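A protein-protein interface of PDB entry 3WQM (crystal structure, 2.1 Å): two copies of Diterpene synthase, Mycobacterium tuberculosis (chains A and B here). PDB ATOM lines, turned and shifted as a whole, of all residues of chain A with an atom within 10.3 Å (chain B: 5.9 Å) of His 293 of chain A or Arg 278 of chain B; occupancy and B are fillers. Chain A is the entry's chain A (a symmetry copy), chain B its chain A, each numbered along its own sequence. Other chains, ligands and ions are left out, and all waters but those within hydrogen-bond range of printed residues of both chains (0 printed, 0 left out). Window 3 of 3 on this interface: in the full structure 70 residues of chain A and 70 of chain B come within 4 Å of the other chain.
Leu 47 of chain A touches Leu 275 of chain B. Leu 47 of chain A touches Tyr 279 of chain B. Tyr 279 of chain B touches Val 234 of chain A (CE1 to O, 3.4 Å). Ala 235 of chain A touches Tyr 279 of chain B. Pro 236 of chain A touches Tyr 279 of chain B. CD2 of Tyr 279 of chain B touches OH of Tyr 239 of chain A, at 3.99 Å. Ile 296 of chain A touches Leu 275 of chain B. Phe 298 of chain A touches Leu 275 of chain B. Phe 298 of chain A touches Arg 278 of chain B (CZ to CD, 3.7 Å). Tyr 279 of chain B touches Phe 298 of chain A (CE1 to CE2, 3.7 Å).
No position is printed for both chains.
His 293 of chain A touches just one residue of chain B: Arg 278 (3.4 Å). Arg 278 of chain B touches just these residues of chain A: His 293 (3.4 Å) and Phe 298 (3.7 Å). No residue of chain A comes within 4 Å of Asn 277 of chain B. Of the printed residues of chain B, Phe 298 of chain A touches Leu 275 (3.96 Å), Arg 278 (3.7 Å) and Tyr 279 (3.7 Å). Printed residues of chain A within 4 Å of Leu 275 of chain B: Leu 47, Ile 296 and Phe 298. Of the printed residues of chain B, Tyr 239 of chain A touches Tyr 279 (3.99 Å). Of the printed residues of chain B, Leu 47 of chain A touches Leu 275, Arg 276 and Tyr 279. Of the printed residues of chain B, Ala 235 of chain A touches Tyr 279 (3.6 Å). Val 274 of chain B touches none of the printed residues of chain A. The nearest residue of chain A that does not touch Arg 278 of chain B is Val 234 of chain A (4.4 Å). The nearest printed residue of chain A that does not touch Arg 280 of chain B is Tyr 239 of chain A (4.4 Å).
Among the printed residues, 15 pairs touch across the chains.
The guanidinium group (NE) of Arg 276 of chain B is in hydrogen-bond range of the backbone carbonyl oxygen (O) of Leu 47 of chain A (2.8 Å). NH2 of Arg 278 of chain B is in hydrogen-bond range of ND1 of His 293 of chain A (3.4 Å).
The side-chain sulfur of Cys 291 of chain A lies within hydrogen-bond range of a ring nitrogen (NE2) of His 293 of chain A. The side-chain amide nitrogen (ND2) of Asn 273 of chain B sits close to the guanidinium group (NH2) of Arg 276 of chain B (3.2 Å). OE1 of Glu 48 of chain A lies close to OH of Tyr 239 of chain A. OG1 of Thr 233 of chain A is in hydrogen-bond range of O of Ala 235 of chain A (2.6 Å). The backbone carbonyl oxygen (O) of Cys 291 of chain A lies within hydrogen-bond range of the backbone NH (N) of Phe 298 of chain A (2.8 Å).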
ATOM      1  N   ARG A  43     -30.770  31.201  -2.122  1.00  0.00           N
ATOM      2  CA  ARG A  43     -30.335  29.901  -2.604  1.00  0.00           C
ATOM      3  C   ARG A  43     -31.338  29.281  -3.565  1.00  0.00           C
ATOM      4  O   ARG A  43     -30.952  28.577  -4.498  1.00  0.00           O
ATOM      5  CB  ARG A  43     -30.059  28.956  -1.431  1.00  0.00           C
ATOM      6  CG  ARG A  43     -31.265  28.271  -0.853  1.00  0.00           C
ATOM      7  CD  ARG A  43     -30.915  27.705   0.503  1.00  0.00           C
ATOM      8  NE  ARG A  43     -30.833  28.768   1.498  1.00  0.00           N
ATOM      9  CZ  ARG A  43     -30.572  28.574   2.783  1.00  0.00           C
ATOM     10  NH1 ARG A  43     -30.354  27.350   3.242  1.00  0.00           N
ATOM     11  NH2 ARG A  43     -30.556  29.606   3.616  1.00  0.00           N
ATOM     12  N   LEU A  47     -30.306  28.488  -7.351  1.00  0.00           N
ATOM     13  CA  LEU A  47     -30.326  27.049  -7.598  1.00  0.00           C
ATOM     14  C   LEU A  47     -31.410  26.578  -8.569  1.00  0.00           C
ATOM     15  O   LEU A  47     -31.175  25.674  -9.367  1.00  0.00           O
ATOM     16  CB  LEU A  47     -30.466  26.287  -6.274  1.00  0.00           C
ATOM     17  CG  LEU A  47     -29.277  26.345  -5.308  1.00  0.00           C
ATOM     18  CD1 LEU A  47     -29.658  25.721  -3.975  1.00  0.00           C
ATOM     19  CD2 LEU A  47     -28.085  25.621  -5.921  1.00  0.00           C
ATOM     20  N   GLU A  48     -32.590  27.189  -8.513  1.00  0.00           N
ATOM     21  CA  GLU A  48     -33.687  26.776  -9.387  1.00  0.00           C
ATOM     22  C   GLU A  48     -34.055  27.723 -10.521  1.00  0.00           C
ATOM     23  O   GLU A  48     -34.863  27.375 -11.383  1.00  0.00           O
ATOM     24  CB  GLU A  48     -34.932  26.489  -8.550  1.00  0.00           C
ATOM     25  CG  GLU A  48     -34.767  25.286  -7.652  1.00  0.00           C
ATOM     26  CD  GLU A  48     -34.509  24.013  -8.434  1.00  0.00           C
ATOM     27  OE1 GLU A  48     -34.006  23.038  -7.837  1.00  0.00           O
ATOM     28  OE2 GLU A  48     -34.816  23.987  -9.645  1.00  0.00           O
ATOM     29  N   THR A 233     -39.506  20.982   5.788  1.00  0.00           N
ATOM     30  CA  THR A 233     -39.143  20.419   4.493  1.00  0.00           C
ATOM     31  C   THR A 233     -37.619  20.473   4.390  1.00  0.00           C
ATOM     32  O   THR A 233     -36.964  21.206   5.129  1.00  0.00           O
ATOM     33  CB  THR A 233     -39.760  21.231   3.324  1.00  0.00           C
ATOM     34  OG1 THR A 233     -39.268  22.577   3.360  1.00  0.00           O
ATOM     35  CG2 THR A 233     -41.290  21.272   3.442  1.00  0.00           C
ATOM     36  N   VAL A 234     -37.049  19.677   3.497  1.00  0.00           N
ATOM     37  CA  VAL A 234     -35.607  19.690   3.327  1.00  0.00           C
ATOM     38  C   VAL A 234     -35.194  20.935   2.533  1.00  0.00           C
ATOM     39  O   VAL A 234     -34.236  21.620   2.889  1.00  0.00           O
ATOM     40  CB  VAL A 234     -35.130  18.420   2.597  1.00  0.00           C
ATOM     41  CG1 VAL A 234     -33.637  18.524   2.278  1.00  0.00           C
ATOM     42  CG2 VAL A 234     -35.400  17.205   3.467  1.00  0.00           C
ATOM     43  N   ALA A 235     -35.944  21.231   1.477  1.00  0.00           N
ATOM     44  CA  ALA A 235     -35.672  22.384   0.620  1.00  0.00           C
ATOM     45  C   ALA A 235     -36.406  23.644   1.078  1.00  0.00           C
ATOM     46  O   ALA A 235     -37.421  23.567   1.764  1.00  0.00           O
ATOM     47  CB  ALA A 235     -36.062  22.057  -0.819  1.00  0.00           C
ATOM     48  N   PRO A 236     -35.901  24.824   0.678  1.00  0.00           N
ATOM     49  CA  PRO A 236     -36.486  26.124   1.030  1.00  0.00           C
ATOM     50  C   PRO A 236     -37.972  26.250   0.676  1.00  0.00           C
ATOM     51  O   PRO A 236     -38.492  25.529  -0.178  1.00  0.00           O
ATOM     52  CB  PRO A 236     -35.621  27.116   0.250  1.00  0.00           C
ATOM     53  CG  PRO A 236     -34.285  26.426   0.194  1.00  0.00           C
ATOM     54  CD  PRO A 236     -34.676  25.004  -0.127  1.00  0.00           C
ATOM     55  N   TYR A 239     -39.716  25.799  -2.821  1.00  0.00           N
ATOM     56  CA  TYR A 239     -39.740  24.489  -3.474  1.00  0.00           C
ATOM     57  C   TYR A 239     -41.044  23.736  -3.208  1.00  0.00           C
ATOM     58  O   TYR A 239     -41.347  22.750  -3.880  1.00  0.00           O
ATOM     59  CB  TYR A 239     -38.584  23.618  -2.964  1.00  0.00           C
ATOM     60  CG  TYR A 239     -37.216  23.912  -3.551  1.00  0.00           C
ATOM     61  CD1 TYR A 239     -36.715  23.156  -4.610  1.00  0.00           C
ATOM     62  CD2 TYR A 239     -36.405  24.910  -3.013  1.00  0.00           C
ATOM     63  CE1 TYR A 239     -35.431  23.381  -5.116  1.00  0.00           C
ATOM     64  CE2 TYR A 239     -35.119  25.146  -3.512  1.00  0.00           C
ATOM     65  CZ  TYR A 239     -34.640  24.377  -4.561  1.00  0.00           C
ATOM     66  OH  TYR A 239     -33.371  24.602  -5.050  1.00  0.00           O
ATOM     67  N   GLY A 290     -28.521  17.004  12.856  1.00  0.00           N
ATOM     68  CA  GLY A 290     -28.186  16.977  11.445  1.00  0.00           C
ATOM     69  C   GLY A 290     -26.720  16.879  11.096  1.00  0.00           C
ATOM     70  O   GLY A 290     -25.887  16.508  11.913  1.00  0.00           O
ATOM     71  N   CYS A 291     -26.421  17.209   9.846  1.00  0.00           N
ATOM     72  CA  CYS A 291     -25.068  17.190   9.328  1.00  0.00           C
ATOM     73  C   CYS A 291     -24.954  18.419   8.442  1.00  0.00           C
ATOM     74  O   CYS A 291     -25.962  18.922   7.930  1.00  0.00           O
ATOM     75  CB  CYS A 291     -24.833  15.924   8.507  1.00  0.00           C
ATOM     76  SG  CYS A 291     -25.978  15.741   7.135  1.00  0.00           S
ATOM     77  N   VAL A 292     -23.737  18.910   8.265  1.00  0.00           N
ATOM     78  CA  VAL A 292     -23.521  20.096   7.459  1.00  0.00           C
ATOM     79  C   VAL A 292     -22.788  19.781   6.157  1.00  0.00           C
ATOM     80  O   VAL A 292     -21.809  19.028   6.143  1.00  0.00           O
ATOM     81  CB  VAL A 292     -22.721  21.145   8.256  1.00  0.00           C
ATOM     82  CG1 VAL A 292     -22.544  22.426   7.435  1.00  0.00           C
ATOM     83  CG2 VAL A 292     -23.437  21.444   9.566  1.00  0.00           C
ATOM     84  N   HIS A 293     -23.287  20.347   5.063  1.00  0.00           N
ATOM     85  CA  HIS A 293     -22.682  20.170   3.742  1.00  0.00           C
ATOM     86  C   HIS A 293     -22.629  21.555   3.118  1.00  0.00           C
ATOM     87  O   HIS A 293     -23.663  22.213   2.966  1.00  0.00           O
ATOM     88  CB  HIS A 293     -23.525  19.237   2.864  1.00  0.00           C
ATOM     89  CG  HIS A 293     -23.573  17.823   3.355  1.00  0.00           C
ATOM     90  ND1 HIS A 293     -22.472  16.993   3.347  1.00  0.00           N
ATOM     91  CD2 HIS A 293     -24.585  17.098   3.890  1.00  0.00           C
ATOM     92  CE1 HIS A 293     -22.804  15.819   3.855  1.00  0.00           C
ATOM     93  NE2 HIS A 293     -24.081  15.857   4.192  1.00  0.00           N
ATOM     94  N   ASP A 294     -21.424  22.011   2.785  1.00  0.00           N
ATOM     95  CA  ASP A 294     -21.256  23.329   2.185  1.00  0.00           C
ATOM     96  C   ASP A 294     -21.843  24.447   3.027  1.00  0.00           C
ATOM     97  O   ASP A 294     -22.414  25.396   2.491  1.00  0.00           O
ATOM     98  CB  ASP A 294     -21.905  23.357   0.805  1.00  0.00           C
ATOM     99  CG  ASP A 294     -20.927  23.037  -0.293  1.00  0.00           C
ATOM    100  OD1 ASP A 294     -20.025  22.195  -0.060  1.00  0.00           O
ATOM    101  OD2 ASP A 294     -21.064  23.625  -1.387  1.00  0.00           O
ATOM    102  N   GLY A 295     -21.705  24.341   4.342  1.00  0.00           N
ATOM    103  CA  GLY A 295     -22.238  25.371   5.215  1.00  0.00           C
ATOM    104  C   GLY A 295     -23.740  25.268   5.421  1.00  0.00           C
ATOM    105  O   GLY A 295     -24.329  26.054   6.171  1.00  0.00           O
ATOM    106  N   ILE A 296     -24.369  24.303   4.761  1.00  0.00           N
ATOM    107  CA  ILE A 296     -25.809  24.127   4.904  1.00  0.00           C
ATOM    108  C   ILE A 296     -26.125  22.900   5.749  1.00  0.00           C
ATOM    109  O   ILE A 296     -25.619  21.808   5.506  1.00  0.00           O
ATOM    110  CB  ILE A 296     -26.508  24.010   3.525  1.00  0.00           C
ATOM    111  CG1 ILE A 296     -26.263  25.289   2.714  1.00  0.00           C
ATOM    112  CG2 ILE A 296     -28.011  23.819   3.713  1.00  0.00           C
ATOM    113  CD1 ILE A 296     -26.786  25.234   1.299  1.00  0.00           C
ATOM    114  N   TRP A 297     -26.976  23.103   6.746  1.00  0.00           N
ATOM    115  CA  TRP A 297     -27.388  22.042   7.660  1.00  0.00           C
ATOM    116  C   TRP A 297     -28.522  21.216   7.048  1.00  0.00           C
ATOM    117  O   TRP A 297     -29.445  21.770   6.449  1.00  0.00           O
ATOM    118  CB  TRP A 297     -27.855  22.688   8.974  1.00  0.00           C
ATOM    119  CG  TRP A 297     -28.223  21.746  10.078  1.00  0.00           C
ATOM    120  CD1 TRP A 297     -27.446  21.383  11.138  1.00  0.00           C
ATOM    121  CD2 TRP A 297     -29.495  21.119  10.276  1.00  0.00           C
ATOM    122  NE1 TRP A 297     -28.163  20.576  11.999  1.00  0.00           N
ATOM    123  CE2 TRP A 297     -29.424  20.400  11.489  1.00  0.00           C
ATOM    124  CE3 TRP A 297     -30.696  21.102   9.546  1.00  0.00           C
ATOM    125  CZ2 TRP A 297     -30.504  19.674  11.991  1.00  0.00           C
ATOM    126  CZ3 TRP A 297     -31.769  20.378  10.046  1.00  0.00           C
ATOM    127  CH2 TRP A 297     -31.666  19.673  11.261  1.00  0.00           C
ATOM    128  N   PHE A 298     -28.437  19.895   7.180  1.00  0.00           N
ATOM    129  CA  PHE A 298     -29.480  18.995   6.690  1.00  0.00           C
ATOM    130  C   PHE A 298     -29.805  18.019   7.823  1.00  0.00           C
ATOM    131  O   PHE A 298     -28.900  17.500   8.480  1.00  0.00           O
ATOM    132  CB  PHE A 298     -29.022  18.181   5.467  1.00  0.00           C
ATOM    133  CG  PHE A 298     -28.806  19.000   4.214  1.00  0.00           C
ATOM    134  CD1 PHE A 298     -27.640  19.742   4.041  1.00  0.00           C
ATOM    135  CD2 PHE A 298     -29.763  19.010   3.199  1.00  0.00           C
ATOM    136  CE1 PHE A 298     -27.428  20.488   2.867  1.00  0.00           C
ATOM    137  CE2 PHE A 298     -29.562  19.748   2.024  1.00  0.00           C
ATOM    138  CZ  PHE A 298     -28.391  20.487   1.860  1.00  0.00           C
ATOM    139  N   ALA A 299     -31.089  17.775   8.053  1.00  0.00           N
ATOM    140  CA  ALA A 299     -31.519  16.847   9.097  1.00  0.00           C
ATOM    141  C   ALA A 299     -31.184  15.422   8.677  1.00  0.00           C
ATOM    142  O   ALA A 299     -31.359  15.064   7.512  1.00  0.00           O
ATOM    143  CB  ALA A 299     -33.023  16.966   9.315  1.00  0.00           C
ATOM    144  N   GLU A 300     -30.718  14.612   9.625  1.00  0.00           N
ATOM    145  CA  GLU A 300     -30.386  13.212   9.352  1.00  0.00           C
ATOM    146  C   GLU A 300     -31.584  12.311   9.628  1.00  0.00           C
ATOM    147  O   GLU A 300     -32.639  12.770  10.077  1.00  0.00           O
ATOM    148  CB  GLU A 300     -29.243  12.733  10.247  1.00  0.00           C
ATOM    149  CG  GLU A 300     -27.930  13.470  10.077  1.00  0.00           C
ATOM    150  CD  GLU A 300     -26.838  12.893  10.952  1.00  0.00           C
ATOM    151  OE1 GLU A 300     -27.130  12.548  12.116  1.00  0.00           O
ATOM    152  OE2 GLU A 300     -25.684  12.797  10.483  1.00  0.00           O
ATOM    153  N   GLY A 301     -31.399  11.019   9.373  1.00  0.00           N
ATOM    154  CA  GLY A 301     -32.443  10.046   9.634  1.00  0.00           C
ATOM    155  C   GLY A 301     -33.684  10.226   8.795  1.00  0.00           C
ATOM    156  O   GLY A 301     -33.611  10.929   7.760  1.00  0.00           O
ATOM    157  OXT GLY A 301     -34.728   9.648   9.176  1.00  0.00           O
ATOM    158  N   ASN B 273     -23.996  22.437  -7.924  1.00  0.00           N
ATOM    159  CA  ASN B 273     -24.774  21.441  -8.647  1.00  0.00           C
ATOM    160  C   ASN B 273     -25.118  20.251  -7.749  1.00  0.00           C
ATOM    161  O   ASN B 273     -26.202  19.673  -7.847  1.00  0.00           O
ATOM    162  CB  ASN B 273     -23.989  20.966  -9.861  1.00  0.00           C
ATOM    163  CG  ASN B 273     -24.868  20.338 -10.900  1.00  0.00           C
ATOM    164  OD1 ASN B 273     -25.417  19.255 -10.695  1.00  0.00           O
ATOM    165  ND2 ASN B 273     -25.022  21.020 -12.028  1.00  0.00           N
ATOM    166  N   VAL B 274     -24.175  19.879  -6.890  1.00  0.00           N
ATOM    167  CA  VAL B 274     -24.375  18.786  -5.949  1.00  0.00           C
ATOM    168  C   VAL B 274     -25.413  19.249  -4.928  1.00  0.00           C
ATOM    169  O   VAL B 274     -26.256  18.471  -4.475  1.00  0.00           O
ATOM    170  CB  VAL B 274     -23.051  18.439  -5.224  1.00  0.00           C
ATOM    171  CG1 VAL B 274     -23.318  17.526  -4.033  1.00  0.00           C
ATOM    172  CG2 VAL B 274     -22.091  17.765  -6.204  1.00  0.00           C
ATOM    173  N   LEU B 275     -25.340  20.530  -4.578  1.00  0.00           N
ATOM    174  CA  LEU B 275     -26.266  21.132  -3.627  1.00  0.00           C
ATOM    175  C   LEU B 275     -27.664  21.147  -4.222  1.00  0.00           C
ATOM    176  O   LEU B 275     -28.633  20.763  -3.564  1.00  0.00           O
ATOM    177  CB  LEU B 275     -25.834  22.564  -3.299  1.00  0.00           C
ATOM    178  CG  LEU B 275     -26.789  23.390  -2.430  1.00  0.00           C
ATOM    179  CD1 LEU B 275     -26.943  22.731  -1.067  1.00  0.00           C
ATOM    180  CD2 LEU B 275     -26.251  24.811  -2.284  1.00  0.00           C
ATOM    181  N   ARG B 276     -27.767  21.597  -5.468  1.00  0.00           N
ATOM    182  CA  ARG B 276     -29.052  21.647  -6.146  1.00  0.00           C
ATOM    183  C   ARG B 276     -29.671  20.264  -6.134  1.00  0.00           C
ATOM    184  O   ARG B 276     -30.889  20.116  -6.013  1.00  0.00           O
ATOM    185  CB  ARG B 276     -28.890  22.105  -7.596  1.00  0.00           C
ATOM    186  CG  ARG B 276     -30.176  21.993  -8.410  1.00  0.00           C
ATOM    187  CD  ARG B 276     -29.948  22.324  -9.874  1.00  0.00           C
ATOM    188  NE  ARG B 276     -29.352  23.645 -10.033  1.00  0.00           N
ATOM    189  CZ  ARG B 276     -28.161  23.867 -10.577  1.00  0.00           C
ATOM    190  NH1 ARG B 276     -27.700  25.107 -10.675  1.00  0.00           N
ATOM    191  NH2 ARG B 276     -27.435  22.853 -11.032  1.00  0.00           N
ATOM    192  N   ASN B 277     -28.829  19.246  -6.272  1.00  0.00           N
ATOM    193  CA  ASN B 277     -29.318  17.879  -6.281  1.00  0.00           C
ATOM    194  C   ASN B 277     -29.715  17.403  -4.898  1.00  0.00           C
ATOM    195  O   ASN B 277     -30.552  16.518  -4.772  1.00  0.00           O
ATOM    196  CB  ASN B 277     -28.280  16.930  -6.876  1.00  0.00           C
ATOM    197  CG  ASN B 277     -28.104  17.130  -8.364  1.00  0.00           C
ATOM    198  OD1 ASN B 277     -29.026  17.568  -9.055  1.00  0.00           O
ATOM    199  ND2 ASN B 277     -26.924  16.794  -8.872  1.00  0.00           N
ATOM    200  N   ARG B 278     -29.113  17.977  -3.860  1.00  0.00           N
ATOM    201  CA  ARG B 278     -29.463  17.584  -2.499  1.00  0.00           C
ATOM    202  C   ARG B 278     -30.897  18.023  -2.229  1.00  0.00           C
ATOM    203  O   ARG B 278     -31.619  17.367  -1.480  1.00  0.00           O
ATOM    204  CB  ARG B 278     -28.532  18.233  -1.466  1.00  0.00           C
ATOM    205  CG  ARG B 278     -27.148  17.599  -1.342  1.00  0.00           C
ATOM    206  CD  ARG B 278     -26.317  18.307  -0.274  1.00  0.00           C
ATOM    207  NE  ARG B 278     -24.924  17.861  -0.244  1.00  0.00           N
ATOM    208  CZ  ARG B 278     -24.522  16.656   0.149  1.00  0.00           C
ATOM    209  NH1 ARG B 278     -25.404  15.753   0.556  1.00  0.00           N
ATOM    210  NH2 ARG B 278     -23.230  16.352   0.126  1.00  0.00           N
ATOM    211  N   TYR B 279     -31.308  19.129  -2.851  1.00  0.00           N
ATOM    212  CA  TYR B 279     -32.658  19.656  -2.672  1.00  0.00           C
ATOM    213  C   TYR B 279     -33.685  19.034  -3.607  1.00  0.00           C
ATOM    214  O   TYR B 279     -34.847  18.873  -3.236  1.00  0.00           O
ATOM    215  CB  TYR B 279     -32.677  21.174  -2.859  1.00  0.00           C
ATOM    216  CG  TYR B 279     -32.055  21.959  -1.727  1.00  0.00           C
ATOM    217  CD1 TYR B 279     -32.272  21.597  -0.395  1.00  0.00           C
ATOM    218  CD2 TYR B 279     -31.301  23.104  -1.983  1.00  0.00           C
ATOM    219  CE1 TYR B 279     -31.759  22.359   0.653  1.00  0.00           C
ATOM    220  CE2 TYR B 279     -30.784  23.874  -0.946  1.00  0.00           C
ATOM    221  CZ  TYR B 279     -31.018  23.499   0.373  1.00  0.00           C
ATOM    222  OH  TYR B 279     -30.533  24.285   1.401  1.00  0.00           O
ATOM    223  N   ARG B 280     -33.263  18.696  -4.820  1.00  0.00           N
ATOM    224  CA  ARG B 280     -34.163  18.091  -5.795  1.00  0.00           C
ATOM    225  C   ARG B 280     -34.157  16.571  -5.704  1.00  0.00           C
ATOM    226  O   ARG B 280     -35.024  15.907  -6.274  1.00  0.00           O
ATOM    227  CB  ARG B 280     -33.770  18.518  -7.211  1.00  0.00           C
ATOM    228  CG  ARG B 280     -34.079  19.969  -7.541  1.00  0.00           C
ATOM    229  CD  ARG B 280     -33.386  20.380  -8.832  1.00  0.00           C
ATOM    230  NE  ARG B 280     -33.669  19.456  -9.927  1.00  0.00           N
ATOM    231  CZ  ARG B 280     -33.036  19.468 -11.097  1.00  0.00           C
ATOM    232  NH1 ARG B 280     -32.079  20.360 -11.328  1.00  0.00           N
ATOM    233  NH2 ARG B 280     -33.357  18.588 -12.038  1.00  0.00           N
ATOM    234  N   ALA B 281     -33.176  16.027  -4.987  1.00  0.00           N
ATOM    235  CA  ALA B 281     -33.043  14.582  -4.808  1.00  0.00           C
ATOM    236  C   ALA B 281     -34.407  13.978  -4.519  1.00  0.00           C
ATOM    237  O   ALA B 281     -34.991  13.285  -5.354  1.00  0.00           O
ATOM    238  CB  ALA B 281     -32.088  14.286  -3.654  1.00  0.00           C
ATOM    239  N   GLN B 282     -34.893  14.245  -3.312  1.00  0.00           N
ATOM    240  CA  GLN B 282     -36.195  13.789  -2.854  1.00  0.00           C
ATOM    241  C   GLN B 282     -37.012  15.076  -2.746  1.00  0.00           C
ATOM    242  O   GLN B 282     -37.149  15.652  -1.664  1.00  0.00           O
ATOM    243  CB  GLN B 282     -36.055  13.114  -1.488  1.00  0.00           C
ATOM    244  CG  GLN B 282     -35.242  11.823  -1.523  1.00  0.00           C
ATOM    245  CD  GLN B 282     -34.692  11.432  -0.160  1.00  0.00           C
ATOM    246  OE1 GLN B 282     -33.739  12.037   0.336  1.00  0.00           O
ATOM    247  NE2 GLN B 282     -35.296  10.423   0.454  1.00  0.00           N
